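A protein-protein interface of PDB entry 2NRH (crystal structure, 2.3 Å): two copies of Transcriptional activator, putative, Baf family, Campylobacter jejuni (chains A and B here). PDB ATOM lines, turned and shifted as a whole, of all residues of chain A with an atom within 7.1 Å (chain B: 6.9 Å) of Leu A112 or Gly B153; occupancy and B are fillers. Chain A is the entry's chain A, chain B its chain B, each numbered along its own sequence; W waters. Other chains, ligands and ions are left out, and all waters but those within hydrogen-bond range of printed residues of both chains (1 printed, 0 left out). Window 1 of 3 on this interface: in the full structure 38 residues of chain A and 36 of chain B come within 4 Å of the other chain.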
ATOM      1  N   ASP A  91      10.133   6.542   7.066  1.00  0.00           N
ATOM      2  CA  ASP A  91       9.384   6.272   8.307  1.00  0.00           C
ATOM      3  C   ASP A  91      10.341   5.651   9.308  1.00  0.00           C
ATOM      4  O   ASP A  91      10.814   4.533   9.093  1.00  0.00           O
ATOM      5  CB  ASP A  91       8.233   5.295   8.028  1.00  0.00           C
ATOM      6  CG  ASP A  91       7.355   5.024   9.240  1.00  0.00           C
ATOM      7  OD1 ASP A  91       7.596   5.582  10.335  1.00  0.00           O
ATOM      8  OD2 ASP A  91       6.386   4.231   9.092  1.00  0.00           O
ATOM      9  N   GLY A  93      11.059   4.070  12.844  1.00  0.00           N
ATOM     10  CA  GLY A  93      10.557   3.403  14.032  1.00  0.00           C
ATOM     11  C   GLY A  93      11.477   2.221  14.330  1.00  0.00           C
ATOM     12  O   GLY A  93      12.712   2.370  14.269  1.00  0.00           O
ATOM     13  N   SER A  94      10.876   1.069  14.665  1.00  0.00           N
ATOM     14  CA  SER A  94      11.554  -0.262  14.757  1.00  0.00           C
ATOM     15  C   SER A  94      12.504  -0.502  13.622  1.00  0.00           C
ATOM     16  O   SER A  94      13.607  -1.000  13.831  1.00  0.00           O
ATOM     17  CB  SER A  94      10.539  -1.402  14.646  1.00  0.00           C
ATOM     18  OG  SER A  94       9.638  -1.272  15.694  1.00  0.00           O
ATOM     19  N   ALA A  95      12.033  -0.155  12.438  1.00  0.00           N
ATOM     20  CA  ALA A  95      12.830  -0.148  11.237  1.00  0.00           C
ATOM     21  C   ALA A  95      12.727   1.248  10.622  1.00  0.00           C
ATOM     22  O   ALA A  95      11.888   2.082  11.005  1.00  0.00           O
ATOM     23  CB  ALA A  95      12.293  -1.247  10.208  1.00  0.00           C
ATOM     24  N   ILE A  96      13.564   1.515   9.647  1.00  0.00           N
ATOM     25  CA  ILE A  96      13.472   2.772   8.969  1.00  0.00           C
ATOM     26  C   ILE A  96      13.287   2.442   7.491  1.00  0.00           C
ATOM     27  O   ILE A  96      14.178   1.885   6.860  1.00  0.00           O
ATOM     28  CB  ILE A  96      14.762   3.613   9.169  1.00  0.00           C
ATOM     29  CG1 ILE A  96      15.001   3.922  10.642  1.00  0.00           C
ATOM     30  CG2 ILE A  96      14.748   4.886   8.275  1.00  0.00           C
ATOM     31  CD1 ILE A  96      16.441   4.351  10.918  1.00  0.00           C
ATOM     32  N   THR A  97      12.114   2.791   6.966  1.00  0.00           N
ATOM     33  CA  THR A  97      11.796   2.487   5.582  1.00  0.00           C
ATOM     34  C   THR A  97      12.000   3.761   4.790  1.00  0.00           C
ATOM     35  O   THR A  97      11.591   4.822   5.230  1.00  0.00           O
ATOM     36  CB  THR A  97      10.354   2.018   5.437  1.00  0.00           C
ATOM     37  OG1 THR A  97       9.472   3.114   5.732  1.00  0.00           O
ATOM     38  CG2 THR A  97      10.045   0.852   6.397  1.00  0.00           C
ATOM     39  N   ILE A  98      12.686   3.647   3.668  1.00  0.00           N
ATOM     40  CA  ILE A  98      12.914   4.771   2.777  1.00  0.00           C
ATOM     41  C   ILE A  98      12.316   4.447   1.394  1.00  0.00           C
ATOM     42  O   ILE A  98      12.814   3.556   0.689  1.00  0.00           O
ATOM     43  CB  ILE A  98      14.412   5.077   2.677  1.00  0.00           C
ATOM     44  CG1 ILE A  98      14.911   5.504   4.040  1.00  0.00           C
ATOM     45  CG2 ILE A  98      14.701   6.166   1.626  1.00  0.00           C
ATOM     46  CD1 ILE A  98      16.224   4.891   4.403  1.00  0.00           C
ATOM     47  N   PHE A 110      13.965   0.956   0.440  1.00  0.00           N
ATOM     48  CA  PHE A 110      14.917   0.090   1.165  1.00  0.00           C
ATOM     49  C   PHE A 110      14.682   0.205   2.656  1.00  0.00           C
ATOM     50  O   PHE A 110      13.898   1.052   3.097  1.00  0.00           O
ATOM     51  CB  PHE A 110      16.398   0.284   0.704  1.00  0.00           C
ATOM     52  CG  PHE A 110      16.927   1.699   0.859  1.00  0.00           C
ATOM     53  CD1 PHE A 110      17.752   2.040   1.947  1.00  0.00           C
ATOM     54  CD2 PHE A 110      16.597   2.691  -0.070  1.00  0.00           C
ATOM     55  CE1 PHE A 110      18.228   3.352   2.094  1.00  0.00           C
ATOM     56  CE2 PHE A 110      17.075   4.015   0.061  1.00  0.00           C
ATOM     57  CZ  PHE A 110      17.898   4.344   1.131  1.00  0.00           C
ATOM     58  N   ILE A 111      15.266  -0.707   3.429  1.00  0.00           N
ATOM     59  CA  ILE A 111      14.930  -0.779   4.853  1.00  0.00           C
ATOM     60  C   ILE A 111      16.186  -0.811   5.681  1.00  0.00           C
ATOM     61  O   ILE A 111      17.179  -1.494   5.321  1.00  0.00           O
ATOM     62  CB  ILE A 111      14.132  -2.035   5.175  1.00  0.00           C
ATOM     63  CG1 ILE A 111      12.792  -2.031   4.419  1.00  0.00           C
ATOM     64  CG2 ILE A 111      13.905  -2.215   6.718  1.00  0.00           C
ATOM     65  CD1 ILE A 111      12.171  -3.445   4.243  1.00  0.00           C
ATOM     66  N   LEU A 112      16.137  -0.122   6.817  1.00  0.00           N
ATOM     67  CA  LEU A 112      17.185  -0.288   7.853  1.00  0.00           C
ATOM     68  C   LEU A 112      16.650  -0.642   9.255  1.00  0.00           C
ATOM     69  O   LEU A 112      15.488  -0.443   9.539  1.00  0.00           O
ATOM     70  CB  LEU A 112      17.912   1.050   7.979  1.00  0.00           C
ATOM     71  CG  LEU A 112      18.464   1.641   6.701  1.00  0.00           C
ATOM     72  CD1 LEU A 112      18.521   3.166   6.907  1.00  0.00           C
ATOM     73  CD2 LEU A 112      19.839   0.985   6.471  1.00  0.00           C
ATOM     74  N   PRO A 113      17.529  -1.080  10.174  1.00  0.00           N
ATOM     75  CA  PRO A 113      17.009  -1.197  11.535  1.00  0.00           C
ATOM     76  C   PRO A 113      16.736   0.192  12.137  1.00  0.00           C
ATOM     77  O   PRO A 113      17.388   1.169  11.769  1.00  0.00           O
ATOM     78  CB  PRO A 113      18.142  -1.882  12.312  1.00  0.00           C
ATOM     79  CG  PRO A 113      19.256  -2.203  11.310  1.00  0.00           C
ATOM     80  CD  PRO A 113      18.963  -1.450  10.054  1.00  0.00           C
ATOM     81  N   GLY A 114      15.766   0.263  13.049  1.00  0.00           N
ATOM     82  CA  GLY A 114      15.503   1.458  13.767  1.00  0.00           C
ATOM     83  C   GLY A 114      16.671   1.691  14.697  1.00  0.00           C
ATOM     84  O   GLY A 114      17.480   0.790  14.951  1.00  0.00           O
ATOM     85  N   ILE A 115      16.758   2.920  15.189  1.00  0.00           N
ATOM     86  CA  ILE A 115      17.878   3.383  15.988  1.00  0.00           C
ATOM     87  C   ILE A 115      18.031   2.597  17.295  1.00  0.00           C
ATOM     88  O   ILE A 115      19.146   2.249  17.655  1.00  0.00           O
ATOM     89  CB  ILE A 115      17.780   4.925  16.251  1.00  0.00           C
ATOM     90  CG1 ILE A 115      18.029   5.653  14.934  1.00  0.00           C
ATOM     91  CG2 ILE A 115      18.770   5.343  17.377  1.00  0.00           C
ATOM     92  CD1 ILE A 115      17.427   7.023  14.889  1.00  0.00           C
ATOM     93  N   TYR A 118      19.593  -0.760  16.442  1.00  0.00           N
ATOM     94  CA  TYR A 118      21.070  -0.576  16.468  1.00  0.00           C
ATOM     95  C   TYR A 118      21.638  -0.608  17.885  1.00  0.00           C
ATOM     96  O   TYR A 118      22.669  -1.208  18.095  1.00  0.00           O
ATOM     97  CB  TYR A 118      21.515   0.727  15.848  1.00  0.00           C
ATOM     98  CG  TYR A 118      21.540   0.728  14.351  1.00  0.00           C
ATOM     99  CD1 TYR A 118      22.621   0.179  13.627  1.00  0.00           C
ATOM    100  CD2 TYR A 118      20.478   1.296  13.656  1.00  0.00           C
ATOM    101  CE1 TYR A 118      22.627   0.204  12.259  1.00  0.00           C
ATOM    102  CE2 TYR A 118      20.483   1.354  12.284  1.00  0.00           C
ATOM    103  CZ  TYR A 118      21.528   0.809  11.600  1.00  0.00           C
ATOM    104  OH  TYR A 118      21.407   0.925  10.256  1.00  0.00           O
ATOM    105  N   VAL A 154      25.805   4.765  13.003  1.00  0.00           N
ATOM    106  CA  VAL A 154      24.340   4.841  12.928  1.00  0.00           C
ATOM    107  C   VAL A 154      23.836   6.106  12.254  1.00  0.00           C
ATOM    108  O   VAL A 154      23.353   6.033  11.113  1.00  0.00           O
ATOM    109  CB  VAL A 154      23.640   4.607  14.324  1.00  0.00           C
ATOM    110  CG1 VAL A 154      22.131   4.651  14.186  1.00  0.00           C
ATOM    111  CG2 VAL A 154      24.002   3.227  14.866  1.00  0.00           C
ATOM    112  N   GLY A 157      25.297   6.936   8.710  1.00  0.00           N
ATOM    113  CA  GLY A 157      24.939   5.877   7.746  1.00  0.00           C
ATOM    114  C   GLY A 157      23.567   6.104   7.174  1.00  0.00           C
ATOM    115  O   GLY A 157      23.368   6.051   5.951  1.00  0.00           O
ATOM    116  N   ILE A 158      22.639   6.432   8.060  1.00  0.00           N
ATOM    117  CA  ILE A 158      21.300   6.757   7.715  1.00  0.00           C
ATOM    118  C   ILE A 158      21.288   8.064   6.876  1.00  0.00           C
ATOM    119  O   ILE A 158      20.704   8.103   5.774  1.00  0.00           O
ATOM    120  CB  ILE A 158      20.495   6.923   9.003  1.00  0.00           C
ATOM    121  CG1 ILE A 158      20.403   5.597   9.767  1.00  0.00           C
ATOM    122  CG2 ILE A 158      19.090   7.479   8.718  1.00  0.00           C
ATOM    123  CD1 ILE A 158      19.744   5.713  11.107  1.00  0.00           C
ATOM    124  N   TYR A 159      21.969   9.106   7.382  1.00  0.00           N
ATOM    125  CA  TYR A 159      22.093  10.365   6.705  1.00  0.00           C
ATOM    126  C   TYR A 159      22.586  10.220   5.298  1.00  0.00           C
ATOM    127  O   TYR A 159      21.962  10.740   4.389  1.00  0.00           O
ATOM    128  CB  TYR A 159      23.013  11.333   7.487  1.00  0.00           C
ATOM    129  CG  TYR A 159      23.230  12.608   6.743  1.00  0.00           C
ATOM    130  CD1 TYR A 159      22.223  13.570   6.688  1.00  0.00           C
ATOM    131  CD2 TYR A 159      24.410  12.836   6.043  1.00  0.00           C
ATOM    132  CE1 TYR A 159      22.384  14.733   5.971  1.00  0.00           C
ATOM    133  CE2 TYR A 159      24.603  14.026   5.327  1.00  0.00           C
ATOM    134  CZ  TYR A 159      23.569  14.967   5.299  1.00  0.00           C
ATOM    135  OH  TYR A 159      23.714  16.146   4.595  1.00  0.00           O
ATOM    136  N   LEU A 161      22.435   7.656   3.340  1.00  0.00           N
ATOM    137  CA  LEU A 161      21.542   6.836   2.507  1.00  0.00           C
ATOM    138  C   LEU A 161      20.340   7.585   1.984  1.00  0.00           C
ATOM    139  O   LEU A 161      20.009   7.476   0.822  1.00  0.00           O
ATOM    140  CB  LEU A 161      21.069   5.587   3.271  1.00  0.00           C
ATOM    141  CG  LEU A 161      21.980   4.374   3.043  1.00  0.00           C
ATOM    142  CD1 LEU A 161      21.852   3.330   4.210  1.00  0.00           C
ATOM    143  CD2 LEU A 161      21.749   3.754   1.665  1.00  0.00           C
ATOM    144  N   ILE A 162      19.666   8.285   2.883  1.00  0.00           N
ATOM    145  CA  ILE A 162      18.619   9.214   2.549  1.00  0.00           C
ATOM    146  C   ILE A 162      19.120  10.313   1.583  1.00  0.00           C
ATOM    147  O   ILE A 162      18.590  10.445   0.484  1.00  0.00           O
ATOM    148  CB  ILE A 162      17.998   9.809   3.830  1.00  0.00           C
ATOM    149  CG1 ILE A 162      17.375   8.696   4.711  1.00  0.00           C
ATOM    150  CG2 ILE A 162      16.927  10.874   3.485  1.00  0.00           C
ATOM    151  CD1 ILE A 162      17.003   9.230   6.088  1.00  0.00           C
ATOM    152  N   TYR B 118      23.657  -7.498  11.306  1.00  0.00           N
ATOM    153  CA  TYR B 118      22.550  -6.842  10.573  1.00  0.00           C
ATOM    154  C   TYR B 118      21.434  -7.855  10.273  1.00  0.00           C
ATOM    155  O   TYR B 118      20.279  -7.555  10.506  1.00  0.00           O
ATOM    156  CB  TYR B 118      23.031  -6.257   9.238  1.00  0.00           C
ATOM    157  CG  TYR B 118      23.654  -4.886   9.300  1.00  0.00           C
ATOM    158  CD1 TYR B 118      22.863  -3.730   9.490  1.00  0.00           C
ATOM    159  CD2 TYR B 118      25.035  -4.712   9.079  1.00  0.00           C
ATOM    160  CE1 TYR B 118      23.462  -2.438   9.514  1.00  0.00           C
ATOM    161  CE2 TYR B 118      25.632  -3.400   9.089  1.00  0.00           C
ATOM    162  CZ  TYR B 118      24.827  -2.282   9.301  1.00  0.00           C
ATOM    163  OH  TYR B 118      25.401  -0.978   9.290  1.00  0.00           O
ATOM    164  N   TYR B 122      17.454  -7.683  11.869  1.00  0.00           N
ATOM    165  CA  TYR B 122      16.271  -7.685  10.982  1.00  0.00           C
ATOM    166  C   TYR B 122      15.260  -8.754  11.438  1.00  0.00           C
ATOM    167  O   TYR B 122      14.069  -8.451  11.714  1.00  0.00           O
ATOM    168  CB  TYR B 122      16.673  -7.901   9.528  1.00  0.00           C
ATOM    169  CG  TYR B 122      17.213  -6.660   8.854  1.00  0.00           C
ATOM    170  CD1 TYR B 122      16.582  -5.394   9.014  1.00  0.00           C
ATOM    171  CD2 TYR B 122      18.327  -6.730   8.025  1.00  0.00           C
ATOM    172  CE1 TYR B 122      17.062  -4.239   8.350  1.00  0.00           C
ATOM    173  CE2 TYR B 122      18.805  -5.602   7.379  1.00  0.00           C
ATOM    174  CZ  TYR B 122      18.184  -4.347   7.557  1.00  0.00           C
ATOM    175  OH  TYR B 122      18.699  -3.242   6.847  1.00  0.00           O
ATOM    176  N   ILE B 125      13.636  -7.812  14.598  1.00  0.00           N
ATOM    177  CA  ILE B 125      12.551  -6.867  14.324  1.00  0.00           C
ATOM    178  C   ILE B 125      11.253  -7.564  13.785  1.00  0.00           C
ATOM    179  O   ILE B 125      10.149  -7.347  14.279  1.00  0.00           O
ATOM    180  CB  ILE B 125      13.003  -5.703  13.390  1.00  0.00           C
ATOM    181  CG1 ILE B 125      14.182  -4.910  14.001  1.00  0.00           C
ATOM    182  CG2 ILE B 125      11.809  -4.734  13.155  1.00  0.00           C
ATOM    183  CD1 ILE B 125      14.996  -4.049  12.987  1.00  0.00           C
ATOM    184  N   LEU B 129      11.205  -9.532   7.849  1.00  0.00           N
ATOM    185  CA  LEU B 129      12.563  -9.097   7.505  1.00  0.00           C
ATOM    186  C   LEU B 129      13.606 -10.201   7.766  1.00  0.00           C
ATOM    187  O   LEU B 129      14.805  -9.996   7.515  1.00  0.00           O
ATOM    188  CB  LEU B 129      12.906  -7.794   8.233  1.00  0.00           C
ATOM    189  CG  LEU B 129      11.751  -6.762   8.311  1.00  0.00           C
ATOM    190  CD1 LEU B 129      12.167  -5.581   9.188  1.00  0.00           C
ATOM    191  CD2 LEU B 129      11.283  -6.255   6.904  1.00  0.00           C
ATOM    192  N   VAL B 137      23.053  -7.863  -5.144  1.00  0.00           N
ATOM    193  CA  VAL B 137      22.156  -6.704  -5.260  1.00  0.00           C
ATOM    194  C   VAL B 137      22.922  -5.517  -5.870  1.00  0.00           C
ATOM    195  O   VAL B 137      24.098  -5.287  -5.567  1.00  0.00           O
ATOM    196  CB  VAL B 137      21.484  -6.317  -3.890  1.00  0.00           C
ATOM    197  CG1 VAL B 137      22.441  -5.541  -2.969  1.00  0.00           C
ATOM    198  CG2 VAL B 137      20.192  -5.522  -4.095  1.00  0.00           C
ATOM    199  N   LEU B 139      23.699  -1.510  -6.441  1.00  0.00           N
ATOM    200  CA  LEU B 139      23.705  -0.338  -5.583  1.00  0.00           C
ATOM    201  C   LEU B 139      23.213   0.904  -6.285  1.00  0.00           C
ATOM    202  O   LEU B 139      22.877   1.903  -5.660  1.00  0.00           O
ATOM    203  CB  LEU B 139      25.086  -0.145  -4.960  1.00  0.00           C
ATOM    204  CG  LEU B 139      25.217  -0.753  -3.542  1.00  0.00           C
ATOM    205  CD1 LEU B 139      24.344  -1.972  -3.213  1.00  0.00           C
ATOM    206  CD2 LEU B 139      26.664  -1.035  -3.184  1.00  0.00           C
ATOM    207  N   PRO B 143      15.614  -0.911  -4.807  1.00  0.00           N
ATOM    208  CA  PRO B 143      15.171  -2.310  -4.773  1.00  0.00           C
ATOM    209  C   PRO B 143      13.662  -2.510  -4.937  1.00  0.00           C
ATOM    210  O   PRO B 143      12.865  -1.629  -4.638  1.00  0.00           O
ATOM    211  CB  PRO B 143      15.667  -2.813  -3.408  1.00  0.00           C
ATOM    212  CG  PRO B 143      16.438  -1.641  -2.770  1.00  0.00           C
ATOM    213  CD  PRO B 143      16.024  -0.409  -3.479  1.00  0.00           C
ATOM    214  N   ASP B 148      16.020  -7.558  -1.317  1.00  0.00           N
ATOM    215  CA  ASP B 148      16.889  -6.565  -1.898  1.00  0.00           C
ATOM    216  C   ASP B 148      16.818  -5.285  -1.091  1.00  0.00           C
ATOM    217  O   ASP B 148      17.818  -4.550  -1.021  1.00  0.00           O
ATOM    218  CB  ASP B 148      16.554  -6.296  -3.389  1.00  0.00           C
ATOM    219  CG  ASP B 148      17.064  -7.390  -4.338  1.00  0.00           C
ATOM    220  OD1 ASP B 148      16.568  -7.414  -5.495  1.00  0.00           O
ATOM    221  OD2 ASP B 148      17.945  -8.226  -3.970  1.00  0.00           O
ATOM    222  N   ALA B 149      15.659  -5.004  -0.497  1.00  0.00           N
ATOM    223  CA  ALA B 149      15.504  -3.804   0.317  1.00  0.00           C
ATOM    224  C   ALA B 149      16.449  -3.804   1.568  1.00  0.00           C
ATOM    225  O   ALA B 149      17.027  -2.754   1.932  1.00  0.00           O
ATOM    226  CB  ALA B 149      14.083  -3.601   0.708  1.00  0.00           C
ATOM    227  N   LEU B 150      16.598  -4.991   2.166  1.00  0.00           N
ATOM    228  CA  LEU B 150      17.575  -5.284   3.206  1.00  0.00           C
ATOM    229  C   LEU B 150      19.025  -5.253   2.735  1.00  0.00           C
ATOM    230  O   LEU B 150      19.913  -4.627   3.377  1.00  0.00           O
ATOM    231  CB  LEU B 150      17.261  -6.648   3.837  1.00  0.00           C
ATOM    232  CG  LEU B 150      15.838  -6.775   4.451  1.00  0.00           C
ATOM    233  CD1 LEU B 150      15.496  -8.229   4.798  1.00  0.00           C
ATOM    234  CD2 LEU B 150      15.508  -5.840   5.649  1.00  0.00           C
ATOM    235  N   SER B 151      19.295  -5.943   1.625  1.00  0.00           N
ATOM    236  CA  SER B 151      20.671  -6.043   1.159  1.00  0.00           C
ATOM    237  C   SER B 151      21.192  -4.699   0.771  1.00  0.00           C
ATOM    238  O   SER B 151      22.359  -4.412   0.989  1.00  0.00           O
ATOM    239  CB  SER B 151      20.806  -7.015   0.010  1.00  0.00           C
ATOM    240  OG  SER B 151      20.039  -8.136   0.338  1.00  0.00           O
ATOM    241  N   TYR B 152      20.306  -3.856   0.228  1.00  0.00           N
ATOM    242  CA  TYR B 152      20.679  -2.530  -0.216  1.00  0.00           C
ATOM    243  C   TYR B 152      20.933  -1.636   0.997  1.00  0.00           C
ATOM    244  O   TYR B 152      21.924  -0.898   1.053  1.00  0.00           O
ATOM    245  CB  TYR B 152      19.583  -1.958  -1.082  1.00  0.00           C
ATOM    246  CG  TYR B 152      19.832  -0.531  -1.594  1.00  0.00           C
ATOM    247  CD1 TYR B 152      20.212  -0.288  -2.932  1.00  0.00           C
ATOM    248  CD2 TYR B 152      19.651   0.572  -0.747  1.00  0.00           C
ATOM    249  CE1 TYR B 152      20.404   1.042  -3.401  1.00  0.00           C
ATOM    250  CE2 TYR B 152      19.827   1.884  -1.193  1.00  0.00           C
ATOM    251  CZ  TYR B 152      20.207   2.108  -2.522  1.00  0.00           C
ATOM    252  OH  TYR B 152      20.372   3.422  -2.924  1.00  0.00           O
ATOM    253  N   GLY B 153      20.025  -1.722   1.963  1.00  0.00           N
ATOM    254  CA  GLY B 153      20.116  -0.916   3.156  1.00  0.00           C
ATOM    255  C   GLY B 153      21.489  -1.131   3.785  1.00  0.00           C
ATOM    256  O   GLY B 153      22.213  -0.186   4.023  1.00  0.00           O
ATOM    257  N   VAL B 154      21.832  -2.386   3.998  1.00  0.00           N
ATOM    258  CA  VAL B 154      23.066  -2.774   4.627  1.00  0.00           C
ATOM    259  C   VAL B 154      24.227  -2.392   3.739  1.00  0.00           C
ATOM    260  O   VAL B 154      25.085  -1.579   4.155  1.00  0.00           O
ATOM    261  CB  VAL B 154      23.070  -4.306   4.988  1.00  0.00           C
ATOM    262  CG1 VAL B 154      24.444  -4.826   5.393  1.00  0.00           C
ATOM    263  CG2 VAL B 154      22.063  -4.569   6.061  1.00  0.00           C
ATOM    264  N   PHE B 155      24.285  -2.969   2.544  1.00  0.00           N
ATOM    265  CA  PHE B 155      25.524  -2.867   1.801  1.00  0.00           C
ATOM    266  C   PHE B 155      25.810  -1.444   1.314  1.00  0.00           C
ATOM    267  O   PHE B 155      26.971  -1.012   1.266  1.00  0.00           O
ATOM    268  CB  PHE B 155      25.599  -3.855   0.640  1.00  0.00           C
ATOM    269  CG  PHE B 155      25.500  -5.297   1.044  1.00  0.00           C
ATOM    270  CD1 PHE B 155      25.922  -5.726   2.294  1.00  0.00           C
ATOM    271  CD2 PHE B 155      24.986  -6.241   0.140  1.00  0.00           C
ATOM    272  CE1 PHE B 155      25.813  -7.078   2.666  1.00  0.00           C
ATOM    273  CE2 PHE B 155      24.870  -7.592   0.488  1.00  0.00           C
ATOM    274  CZ  PHE B 155      25.293  -8.020   1.762  1.00  0.00           C
ATOM    275  N   LYS B 156      24.762  -0.713   0.953  1.00  0.00           N
ATOM    276  CA  LYS B 156      24.967   0.653   0.488  1.00  0.00           C
ATOM    277  C   LYS B 156      25.305   1.625   1.578  1.00  0.00           C
ATOM    278  O   LYS B 156      26.053   2.582   1.315  1.00  0.00           O
ATOM    279  CB  LYS B 156      23.796   1.202  -0.336  1.00  0.00           C
ATOM    280  CG  LYS B 156      24.371   1.994  -1.533  1.00  0.00           C
ATOM    281  CD  LYS B 156      23.570   3.158  -1.988  1.00  0.00           C
ATOM    282  CE  LYS B 156      24.213   3.681  -3.260  1.00  0.00           C
ATOM    283  NZ  LYS B 156      23.272   4.638  -3.976  1.00  0.00           N
ATOM    284  N   GLY B 157      24.730   1.406   2.767  1.00  0.00           N
ATOM    285  CA  GLY B 157      25.085   2.127   3.967  1.00  0.00           C
ATOM    286  C   GLY B 157      26.573   2.050   4.286  1.00  0.00           C
ATOM    287  O   GLY B 157      27.188   3.066   4.603  1.00  0.00           O
ATOM    288  N   ILE B 158      27.144   0.851   4.210  1.00  0.00           N
ATOM    289  CA  ILE B 158      28.593   0.637   4.368  1.00  0.00           C
ATOM    290  C   ILE B 158      29.384   1.232   3.206  1.00  0.00           C
ATOM    291  O   ILE B 158      30.428   1.817   3.426  1.00  0.00           O
ATOM    292  CB  ILE B 158      28.979  -0.902   4.472  1.00  0.00           C
ATOM    293  CG1 ILE B 158      28.319  -1.582   5.663  1.00  0.00           C
ATOM    294  CG2 ILE B 158      30.429  -1.092   4.664  1.00  0.00           C
ATOM    295  CD1 ILE B 158      28.286  -3.055   5.497  1.00  0.00           C
HETATM  296  O   HOH W   1      20.773   5.565  -1.618  1.00  0.00           O
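The side-chain hydroxyl (OH) of Tyr B122 lies within hydrogen-bond range of the backbone carbonyl oxygen (O) of Ile A111 (2.8 Å). O of Ala B149 lies within hydrogen-bond range of N of Ile A111.
O of Ser A94 sits at hydrogen-bond distance from N of Gly A114 (2.6 Å). O of Leu A112 sits at hydrogen-bond distance from N of Ile A96. The backbone carbonyl oxygen (O) of Ile A98 lies within hydrogen-bond range of the backbone NH (N) of Phe A110. O of Leu B139 is in hydrogen-bond range of NZ of Lys B156, 3.2 Å away. The side-chain hydroxyl (OH) of Tyr B152 sits at hydrogen-bond distance from the side-chain amino group (NZ) of Lys B156 (3.3 Å).
Among the printed residues, merely in contact across the chains: Ser A94 with Ile B125, Phe A110 with Pro B143, Phe A110 with Ala B149, Phe A110 with Tyr B152, Phe A110 with Gly B153, Ile A111 with Leu B129, Ile A111 with Gly B153, Leu A112 with Tyr B122, Leu A112 with Gly B153, Pro A113 with Tyr B122, Pro A113 with Ile B125, Tyr A118 with Tyr B118, Leu A161 with Tyr B152, Leu A161 with Gly B153, Leu A161 with Lys B156 and Leu A161 with Gly B157.
Leu A112 touches just these residues of chain B: Tyr B122 and Gly B153. Of the printed residues of chain A, Ile B125 touches Ser A94 (3.5 Å) and Pro A113 (3.8 Å). Of the printed residues of chain A, Pro B143 touches Phe A110 (3.97 Å). Of chain A, only Phe A110 (3.97 Å), Ile A111 (3.7 Å), Leu A112 (3.6 Å) and Leu A161 (3.5 Å) come within 4 Å of Gly B153. The nearest residue of chain A that does not touch Gly B153 is Tyr A118 (6.4 Å). The nearest printed residue of chain B that does not touch Tyr A118 is Tyr B122 (6.0 Å).
Printed residues of chain A that touch a printed residue of chain B: Ser A94, Phe A110, Ile A111, Leu A112, Pro A113, Tyr A118 and Leu A161. Hydrophobic or aromatic side chains of chain A within 4 Å of the printed part of chain B: Phe A110, Ile A111, Leu A112, Pro A113, Tyr A118 and Leu A161. Along chain A the printed residues that touch a printed residue of chain B span positions 94 to 161. Of the 18 printed residues of chain B, 10 touch a printed residue of chain A. Among the printed residues, 18 pairs touch across the chains. Among the printed residues, no Asp or Glu carboxylate lies within 4 Å of a Lys or Arg side-chain nitrogen of the other chain.
Tyr B118 touches its own counterpart, Tyr A118. Positions printed for both chains: 118, 154, 157 and 158. Of the 18 pairs that touch across the chains among the printed residues, 1 has its exchanged pair printed and touching as well.
Water W1 bridges OH of Tyr B152 (2.5 Å) and O of Leu A161 (3.2 Å).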
